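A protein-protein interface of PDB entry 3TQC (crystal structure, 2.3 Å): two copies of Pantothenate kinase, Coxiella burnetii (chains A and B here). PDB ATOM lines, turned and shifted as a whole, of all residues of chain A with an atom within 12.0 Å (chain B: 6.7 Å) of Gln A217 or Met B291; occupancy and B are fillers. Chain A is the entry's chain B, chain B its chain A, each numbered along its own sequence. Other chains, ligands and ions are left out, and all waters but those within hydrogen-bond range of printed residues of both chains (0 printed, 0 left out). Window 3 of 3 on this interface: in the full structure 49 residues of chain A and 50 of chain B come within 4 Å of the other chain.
NH2 of Arg A213 lies within hydrogen-bond range of O of Glu B292 (2.9 Å). The backbone carbonyl oxygen (O) of Pro B296 lies within hydrogen-bond range of the backbone NH (N) of Gln A220 (2.8 Å). O of Glu B292 sits close to O of Leu A216, 3.3 Å away.
The backbone carbonyl oxygen of Leu B290 lies within hydrogen-bond range of the backbone NH of Leu B295 (2.8 Å). The backbone carbonyl oxygen (O) of Val A212 lies close to the side-chain amide oxygen (OE1) of Gln A218, 3.1 Å away. NH2 of Arg A213 is in hydrogen-bond range of O of Leu A216. N of Lys A214 is in hydrogen-bond range of OE1 of Gln A218, at 2.9 Å. OG1 of Thr A215 sits at hydrogen-bond distance from N of Gln A218 (3.3 Å). The side-chain amide oxygen of Gln A218 is in hydrogen-bond range of the side-chain amide nitrogen of Gln A220 (2.8 Å).
Leu A216 touches Pro B296. Gln A217 touches Met B291. Gln A217 touches Pro B296 (O to CG, 3.8 Å). CB of Pro B296 touches O of Gln A218, 3.4 Å away. Leu A219 touches Leu B295 (CD2 to O, 3.99 Å). O of Pro B296 touches CD2 of Leu A219, at 3.4 Å.
Val A212 touches none of the printed residues of chain B. Of the printed residues of chain B, Arg A213 touches Glu B292 (2.9 Å). Gln A217 touches just these residues of chain B: Met B291 and Pro B296. Of the printed residues of chain B, Leu A219 touches Leu B295 and Pro B296. No residue of chain A comes within 4 Å of Ala B237. No residue of chain A comes within 4 Å of Lys B287. No residue of chain A comes within 4 Å of Val B288. No residue of chain A comes within 4 Å of Asn B289. No residue of chain A comes within 4 Å of Leu B290. The nearest residue of chain A that does not touch Met B291 is Leu A216 (4.5 Å). The nearest printed residue of chain A that does not touch Leu B295 is Gln A217 (5.9 Å).
Of the 12 printed residues of chain B, 4 touch a printed residue of chain A. Hydrophobic or aromatic side chains of chain A that line the printed part of chain B: Leu A216 and Leu A219. Among the printed residues, 9 pairs touch across the chains. Among the printed residues, no Asp or Glu carboxylate lies within 4 Å of a Lys or Arg side-chain nitrogen of the other chain.
No position is printed for both chains. Of the 9 pairs that touch across the chains among the printed residues, none has its exchanged pair printed and touching as well.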
ATOM      1  N   GLY A 211      -9.426  -8.745   1.804  1.00  0.00           N
ATOM      2  CA  GLY A 211      -8.950 -10.112   1.978  1.00  0.00           C
ATOM      3  C   GLY A 211      -7.501 -10.139   2.437  1.00  0.00           C
ATOM      4  O   GLY A 211      -6.796  -9.120   2.391  1.00  0.00           O
ATOM      5  N   VAL A 212      -7.049 -11.306   2.881  1.00  0.00           N
ATOM      6  CA  VAL A 212      -5.658 -11.478   3.278  1.00  0.00           C
ATOM      7  C   VAL A 212      -4.817 -11.806   2.032  1.00  0.00           C
ATOM      8  O   VAL A 212      -5.283 -12.514   1.133  1.00  0.00           O
ATOM      9  CB  VAL A 212      -5.525 -12.585   4.350  1.00  0.00           C
ATOM     10  CG1 VAL A 212      -6.540 -12.362   5.464  1.00  0.00           C
ATOM     11  CG2 VAL A 212      -5.715 -13.963   3.739  1.00  0.00           C
ATOM     12  N   ARG A 213      -3.597 -11.284   1.963  1.00  0.00           N
ATOM     13  CA  ARG A 213      -2.705 -11.611   0.844  1.00  0.00           C
ATOM     14  C   ARG A 213      -1.950 -12.890   1.209  1.00  0.00           C
ATOM     15  O   ARG A 213      -0.931 -12.821   1.882  1.00  0.00           O
ATOM     16  CB  ARG A 213      -1.684 -10.488   0.544  1.00  0.00           C
ATOM     17  CG  ARG A 213      -2.182  -9.031   0.592  1.00  0.00           C
ATOM     18  CD  ARG A 213      -2.836  -8.538  -0.697  1.00  0.00           C
ATOM     19  NE  ARG A 213      -1.963  -8.478  -1.880  1.00  0.00           N
ATOM     20  CZ  ARG A 213      -1.168  -7.458  -2.223  1.00  0.00           C
ATOM     21  NH1 ARG A 213      -1.060  -6.376  -1.465  1.00  0.00           N
ATOM     22  NH2 ARG A 213      -0.447  -7.532  -3.336  1.00  0.00           N
ATOM     23  N   LYS A 214      -2.442 -14.058   0.794  1.00  0.00           N
ATOM     24  CA  LYS A 214      -1.668 -15.291   0.985  1.00  0.00           C
ATOM     25  C   LYS A 214      -0.298 -15.079   0.354  1.00  0.00           C
ATOM     26  O   LYS A 214       0.725 -15.234   1.017  1.00  0.00           O
ATOM     27  CB  LYS A 214      -2.352 -16.509   0.359  1.00  0.00           C
ATOM     28  CG  LYS A 214      -3.556 -17.043   1.141  1.00  0.00           C
ATOM     29  CD  LYS A 214      -3.858 -18.505   0.760  1.00  0.00           C
ATOM     30  CE  LYS A 214      -5.336 -18.866   0.944  1.00  0.00           C
ATOM     31  NZ  LYS A 214      -5.610 -20.278   0.521  1.00  0.00           N
ATOM     32  N   THR A 215      -0.301 -14.724  -0.931  1.00  0.00           N
ATOM     33  CA  THR A 215       0.882 -14.209  -1.619  1.00  0.00           C
ATOM     34  C   THR A 215       0.591 -12.808  -2.154  1.00  0.00           C
ATOM     35  O   THR A 215      -0.564 -12.391  -2.249  1.00  0.00           O
ATOM     36  CB  THR A 215       1.324 -15.107  -2.809  1.00  0.00           C
ATOM     37  OG1 THR A 215       0.208 -15.352  -3.671  1.00  0.00           O
ATOM     38  CG2 THR A 215       1.907 -16.440  -2.322  1.00  0.00           C
ATOM     39  N   LEU A 216       1.651 -12.088  -2.503  1.00  0.00           N
ATOM     40  CA  LEU A 216       1.518 -10.798  -3.168  1.00  0.00           C
ATOM     41  C   LEU A 216       0.779 -10.944  -4.500  1.00  0.00           C
ATOM     42  O   LEU A 216      -0.069 -10.121  -4.827  1.00  0.00           O
ATOM     43  CB  LEU A 216       2.897 -10.170  -3.407  1.00  0.00           C
ATOM     44  CG  LEU A 216       3.646  -9.655  -2.174  1.00  0.00           C
ATOM     45  CD1 LEU A 216       5.080  -9.294  -2.529  1.00  0.00           C
ATOM     46  CD2 LEU A 216       2.929  -8.459  -1.544  1.00  0.00           C
ATOM     47  N   GLN A 217       1.087 -12.010  -5.237  1.00  0.00           N
ATOM     48  CA  GLN A 217       0.610 -12.194  -6.602  1.00  0.00           C
ATOM     49  C   GLN A 217      -0.838 -12.655  -6.658  1.00  0.00           C
ATOM     50  O   GLN A 217      -1.492 -12.544  -7.697  1.00  0.00           O
ATOM     51  CB  GLN A 217       1.485 -13.210  -7.346  1.00  0.00           C
ATOM     52  CG  GLN A 217       2.950 -12.782  -7.534  1.00  0.00           C
ATOM     53  CD  GLN A 217       3.904 -13.265  -6.431  1.00  0.00           C
ATOM     54  OE1 GLN A 217       3.483 -13.814  -5.399  1.00  0.00           O
ATOM     55  NE2 GLN A 217       5.204 -13.055  -6.653  1.00  0.00           N
ATOM     56  N   GLN A 218      -1.336 -13.194  -5.553  1.00  0.00           N
ATOM     57  CA  GLN A 218      -2.703 -13.677  -5.494  1.00  0.00           C
ATOM     58  C   GLN A 218      -3.695 -12.588  -5.916  1.00  0.00           C
ATOM     59  O   GLN A 218      -3.580 -11.451  -5.466  1.00  0.00           O
ATOM     60  CB  GLN A 218      -3.002 -14.122  -4.064  1.00  0.00           C
ATOM     61  CG  GLN A 218      -4.424 -14.567  -3.813  1.00  0.00           C
ATOM     62  CD  GLN A 218      -4.722 -14.766  -2.339  1.00  0.00           C
ATOM     63  OE1 GLN A 218      -4.310 -13.972  -1.484  1.00  0.00           O
ATOM     64  NE2 GLN A 218      -5.460 -15.823  -2.036  1.00  0.00           N
ATOM     65  N   LEU A 219      -4.658 -12.948  -6.772  1.00  0.00           N
ATOM     66  CA  LEU A 219      -5.712 -12.021  -7.213  1.00  0.00           C
ATOM     67  C   LEU A 219      -6.569 -11.561  -6.040  1.00  0.00           C
ATOM     68  O   LEU A 219      -6.981 -12.375  -5.202  1.00  0.00           O
ATOM     69  CB  LEU A 219      -6.592 -12.649  -8.307  1.00  0.00           C
ATOM     70  CG  LEU A 219      -6.092 -12.372  -9.734  1.00  0.00           C
ATOM     71  CD1 LEU A 219      -6.525 -13.423 -10.755  1.00  0.00           C
ATOM     72  CD2 LEU A 219      -6.566 -10.986 -10.149  1.00  0.00           C
ATOM     73  N   GLN A 220      -6.820 -10.254  -5.980  1.00  0.00           N
ATOM     74  CA  GLN A 220      -7.515  -9.658  -4.855  1.00  0.00           C
ATOM     75  C   GLN A 220      -8.774  -8.953  -5.319  1.00  0.00           C
ATOM     76  O   GLN A 220      -8.728  -8.036  -6.138  1.00  0.00           O
ATOM     77  CB  GLN A 220      -6.613  -8.662  -4.103  1.00  0.00           C
ATOM     78  CG  GLN A 220      -5.374  -9.277  -3.396  1.00  0.00           C
ATOM     79  CD  GLN A 220      -5.725 -10.344  -2.354  1.00  0.00           C
ATOM     80  OE1 GLN A 220      -6.615 -10.154  -1.518  1.00  0.00           O
ATOM     81  NE2 GLN A 220      -5.031 -11.470  -2.409  1.00  0.00           N
ATOM     82  N   VAL A 221      -9.893  -9.411  -4.778  1.00  0.00           N
ATOM     83  CA  VAL A 221     -11.173  -8.723  -4.862  1.00  0.00           C
ATOM     84  C   VAL A 221     -11.750  -8.664  -3.447  1.00  0.00           C
ATOM     85  O   VAL A 221     -11.524  -9.554  -2.630  1.00  0.00           O
ATOM     86  CB  VAL A 221     -12.180  -9.452  -5.799  1.00  0.00           C
ATOM     87  CG1 VAL A 221     -12.241 -10.946  -5.474  1.00  0.00           C
ATOM     88  CG2 VAL A 221     -13.558  -8.854  -5.665  1.00  0.00           C
ATOM     89  N   PHE A 222     -12.476  -7.594  -3.178  1.00  0.00           N
ATOM     90  CA  PHE A 222     -13.119  -7.375  -1.898  1.00  0.00           C
ATOM     91  C   PHE A 222     -14.611  -7.542  -2.052  1.00  0.00           C
ATOM     92  O   PHE A 222     -15.133  -7.420  -3.155  1.00  0.00           O
ATOM     93  CB  PHE A 222     -12.836  -5.957  -1.416  1.00  0.00           C
ATOM     94  CG  PHE A 222     -11.404  -5.555  -1.549  1.00  0.00           C
ATOM     95  CD1 PHE A 222     -10.394  -6.443  -1.226  1.00  0.00           C
ATOM     96  CD2 PHE A 222     -11.060  -4.288  -1.976  1.00  0.00           C
ATOM     97  CE1 PHE A 222      -9.082  -6.079  -1.341  1.00  0.00           C
ATOM     98  CE2 PHE A 222      -9.737  -3.926  -2.081  1.00  0.00           C
ATOM     99  CZ  PHE A 222      -8.753  -4.829  -1.764  1.00  0.00           C
ATOM    100  N   ALA B 237       2.633  -9.200 -20.254  1.00  0.00           N
ATOM    101  CA  ALA B 237       3.872  -8.635 -19.701  1.00  0.00           C
ATOM    102  C   ALA B 237       4.997  -8.470 -20.745  1.00  0.00           C
ATOM    103  O   ALA B 237       5.673  -7.445 -20.780  1.00  0.00           O
ATOM    104  CB  ALA B 237       4.355  -9.477 -18.523  1.00  0.00           C
ATOM    105  N   ASN B 286       9.844  -2.590 -12.704  1.00  0.00           N
ATOM    106  CA  ASN B 286       8.444  -2.437 -13.149  1.00  0.00           C
ATOM    107  C   ASN B 286       7.652  -3.738 -13.286  1.00  0.00           C
ATOM    108  O   ASN B 286       6.479  -3.780 -12.964  1.00  0.00           O
ATOM    109  CB  ASN B 286       8.382  -1.650 -14.455  1.00  0.00           C
ATOM    110  CG  ASN B 286       9.095  -0.317 -14.362  1.00  0.00           C
ATOM    111  OD1 ASN B 286       9.897   0.024 -15.229  1.00  0.00           O
ATOM    112  ND2 ASN B 286       8.822   0.433 -13.305  1.00  0.00           N
ATOM    113  N   LYS B 287       8.295  -4.800 -13.750  1.00  0.00           N
ATOM    114  CA  LYS B 287       7.640  -6.094 -13.865  1.00  0.00           C
ATOM    115  C   LYS B 287       7.312  -6.689 -12.489  1.00  0.00           C
ATOM    116  O   LYS B 287       6.289  -7.337 -12.337  1.00  0.00           O
ATOM    117  CB  LYS B 287       8.519  -7.072 -14.656  1.00  0.00           C
ATOM    118  CG  LYS B 287       7.832  -8.366 -15.058  1.00  0.00           C
ATOM    119  CD  LYS B 287       8.838  -9.313 -15.690  1.00  0.00           C
ATOM    120  CE  LYS B 287       8.238 -10.669 -16.031  1.00  0.00           C
ATOM    121  NZ  LYS B 287       9.326 -11.634 -16.381  1.00  0.00           N
ATOM    122  N   VAL B 288       8.179  -6.479 -11.502  1.00  0.00           N
ATOM    123  CA  VAL B 288       7.928  -6.973 -10.147  1.00  0.00           C
ATOM    124  C   VAL B 288       6.748  -6.202  -9.578  1.00  0.00           C
ATOM    125  O   VAL B 288       5.830  -6.780  -8.991  1.00  0.00           O
ATOM    126  CB  VAL B 288       9.162  -6.829  -9.238  1.00  0.00           C
ATOM    127  CG1 VAL B 288       8.846  -7.282  -7.823  1.00  0.00           C
ATOM    128  CG2 VAL B 288      10.358  -7.625  -9.806  1.00  0.00           C
ATOM    129  N   ASN B 289       6.760  -4.895  -9.792  1.00  0.00           N
ATOM    130  CA  ASN B 289       5.672  -4.045  -9.366  1.00  0.00           C
ATOM    131  C   ASN B 289       4.358  -4.476 -10.010  1.00  0.00           C
ATOM    132  O   ASN B 289       3.342  -4.627  -9.331  1.00  0.00           O
ATOM    133  CB  ASN B 289       5.969  -2.595  -9.732  1.00  0.00           C
ATOM    134  CG  ASN B 289       5.037  -1.605  -9.032  1.00  0.00           C
ATOM    135  OD1 ASN B 289       4.370  -1.932  -8.059  1.00  0.00           O
ATOM    136  ND2 ASN B 289       5.034  -0.387  -9.505  1.00  0.00           N
ATOM    137  N   LEU B 290       4.388  -4.673 -11.325  1.00  0.00           N
ATOM    138  CA  LEU B 290       3.234  -5.205 -12.036  1.00  0.00           C
ATOM    139  C   LEU B 290       2.692  -6.463 -11.358  1.00  0.00           C
ATOM    140  O   LEU B 290       1.523  -6.512 -10.974  1.00  0.00           O
ATOM    141  CB  LEU B 290       3.604  -5.511 -13.484  1.00  0.00           C
ATOM    142  CG  LEU B 290       2.552  -6.116 -14.403  1.00  0.00           C
ATOM    143  CD1 LEU B 290       1.263  -5.329 -14.321  1.00  0.00           C
ATOM    144  CD2 LEU B 290       3.071  -6.139 -15.826  1.00  0.00           C
ATOM    145  N   MET B 291       3.551  -7.469 -11.191  1.00  0.00           N
ATOM    146  CA  MET B 291       3.098  -8.777 -10.705  1.00  0.00           C
ATOM    147  C   MET B 291       2.675  -8.760  -9.233  1.00  0.00           C
ATOM    148  O   MET B 291       1.770  -9.498  -8.844  1.00  0.00           O
ATOM    149  CB  MET B 291       4.172  -9.843 -10.920  1.00  0.00           C
ATOM    150  CG  MET B 291       4.594 -10.070 -12.384  1.00  0.00           C
ATOM    151  SD  MET B 291       3.245 -10.453 -13.529  1.00  0.00           S
ATOM    152  CE  MET B 291       4.178 -10.914 -15.004  1.00  0.00           C
ATOM    153  N   GLU B 292       3.315  -7.922  -8.424  1.00  0.00           N
ATOM    154  CA  GLU B 292       3.129  -7.958  -6.972  1.00  0.00           C
ATOM    155  C   GLU B 292       2.076  -6.981  -6.519  1.00  0.00           C
ATOM    156  O   GLU B 292       1.408  -7.217  -5.514  1.00  0.00           O
ATOM    157  CB  GLU B 292       4.441  -7.661  -6.230  1.00  0.00           C
ATOM    158  CG  GLU B 292       5.446  -8.816  -6.262  1.00  0.00           C
ATOM    159  CD  GLU B 292       6.710  -8.556  -5.441  1.00  0.00           C
ATOM    160  OE1 GLU B 292       6.956  -7.409  -5.016  1.00  0.00           O
ATOM    161  OE2 GLU B 292       7.478  -9.511  -5.213  1.00  0.00           O
ATOM    162  N   ASN B 293       1.940  -5.879  -7.251  1.00  0.00           N
ATOM    163  CA  ASN B 293       1.153  -4.747  -6.789  1.00  0.00           C
ATOM    164  C   ASN B 293       0.092  -4.227  -7.718  1.00  0.00           C
ATOM    165  O   ASN B 293      -0.790  -3.532  -7.257  1.00  0.00           O
ATOM    166  CB  ASN B 293       2.082  -3.594  -6.462  1.00  0.00           C
ATOM    167  CG  ASN B 293       3.139  -3.989  -5.492  1.00  0.00           C
ATOM    168  OD1 ASN B 293       2.839  -4.554  -4.449  1.00  0.00           O
ATOM    169  ND2 ASN B 293       4.399  -3.704  -5.826  1.00  0.00           N
ATOM    170  N   ILE B 294       0.158  -4.537  -9.008  1.00  0.00           N
ATOM    171  CA  ILE B 294      -0.757  -3.936  -9.967  1.00  0.00           C
ATOM    172  C   ILE B 294      -1.739  -4.974 -10.472  1.00  0.00           C
ATOM    173  O   ILE B 294      -2.942  -4.827 -10.292  1.00  0.00           O
ATOM    174  CB  ILE B 294      -0.004  -3.283 -11.131  1.00  0.00           C
ATOM    175  CG1 ILE B 294       0.944  -2.190 -10.599  1.00  0.00           C
ATOM    176  CG2 ILE B 294      -0.981  -2.690 -12.169  1.00  0.00           C
ATOM    177  CD1 ILE B 294       1.958  -1.710 -11.641  1.00  0.00           C
ATOM    178  N   LEU B 295      -1.212  -6.023 -11.091  1.00  0.00           N
ATOM    179  CA  LEU B 295      -2.032  -7.089 -11.655  1.00  0.00           C
ATOM    180  C   LEU B 295      -3.010  -7.692 -10.658  1.00  0.00           C
ATOM    181  O   LEU B 295      -4.184  -7.894 -10.984  1.00  0.00           O
ATOM    182  CB  LEU B 295      -1.171  -8.217 -12.240  1.00  0.00           C
ATOM    183  CG  LEU B 295      -1.115  -8.337 -13.762  1.00  0.00           C
ATOM    184  CD1 LEU B 295      -0.421  -9.682 -14.158  1.00  0.00           C
ATOM    185  CD2 LEU B 295      -2.511  -8.226 -14.402  1.00  0.00           C
ATOM    186  N   PRO B 296      -2.537  -7.997  -9.442  1.00  0.00           N
ATOM    187  CA  PRO B 296      -3.444  -8.625  -8.505  1.00  0.00           C
ATOM    188  C   PRO B 296      -4.775  -7.877  -8.302  1.00  0.00           C
ATOM    189  O   PRO B 296      -5.761  -8.488  -7.935  1.00  0.00           O
ATOM    190  CB  PRO B 296      -2.626  -8.655  -7.222  1.00  0.00           C
ATOM    191  CG  PRO B 296      -1.245  -8.799  -7.709  1.00  0.00           C
ATOM    192  CD  PRO B 296      -1.187  -7.878  -8.873  1.00  0.00           C
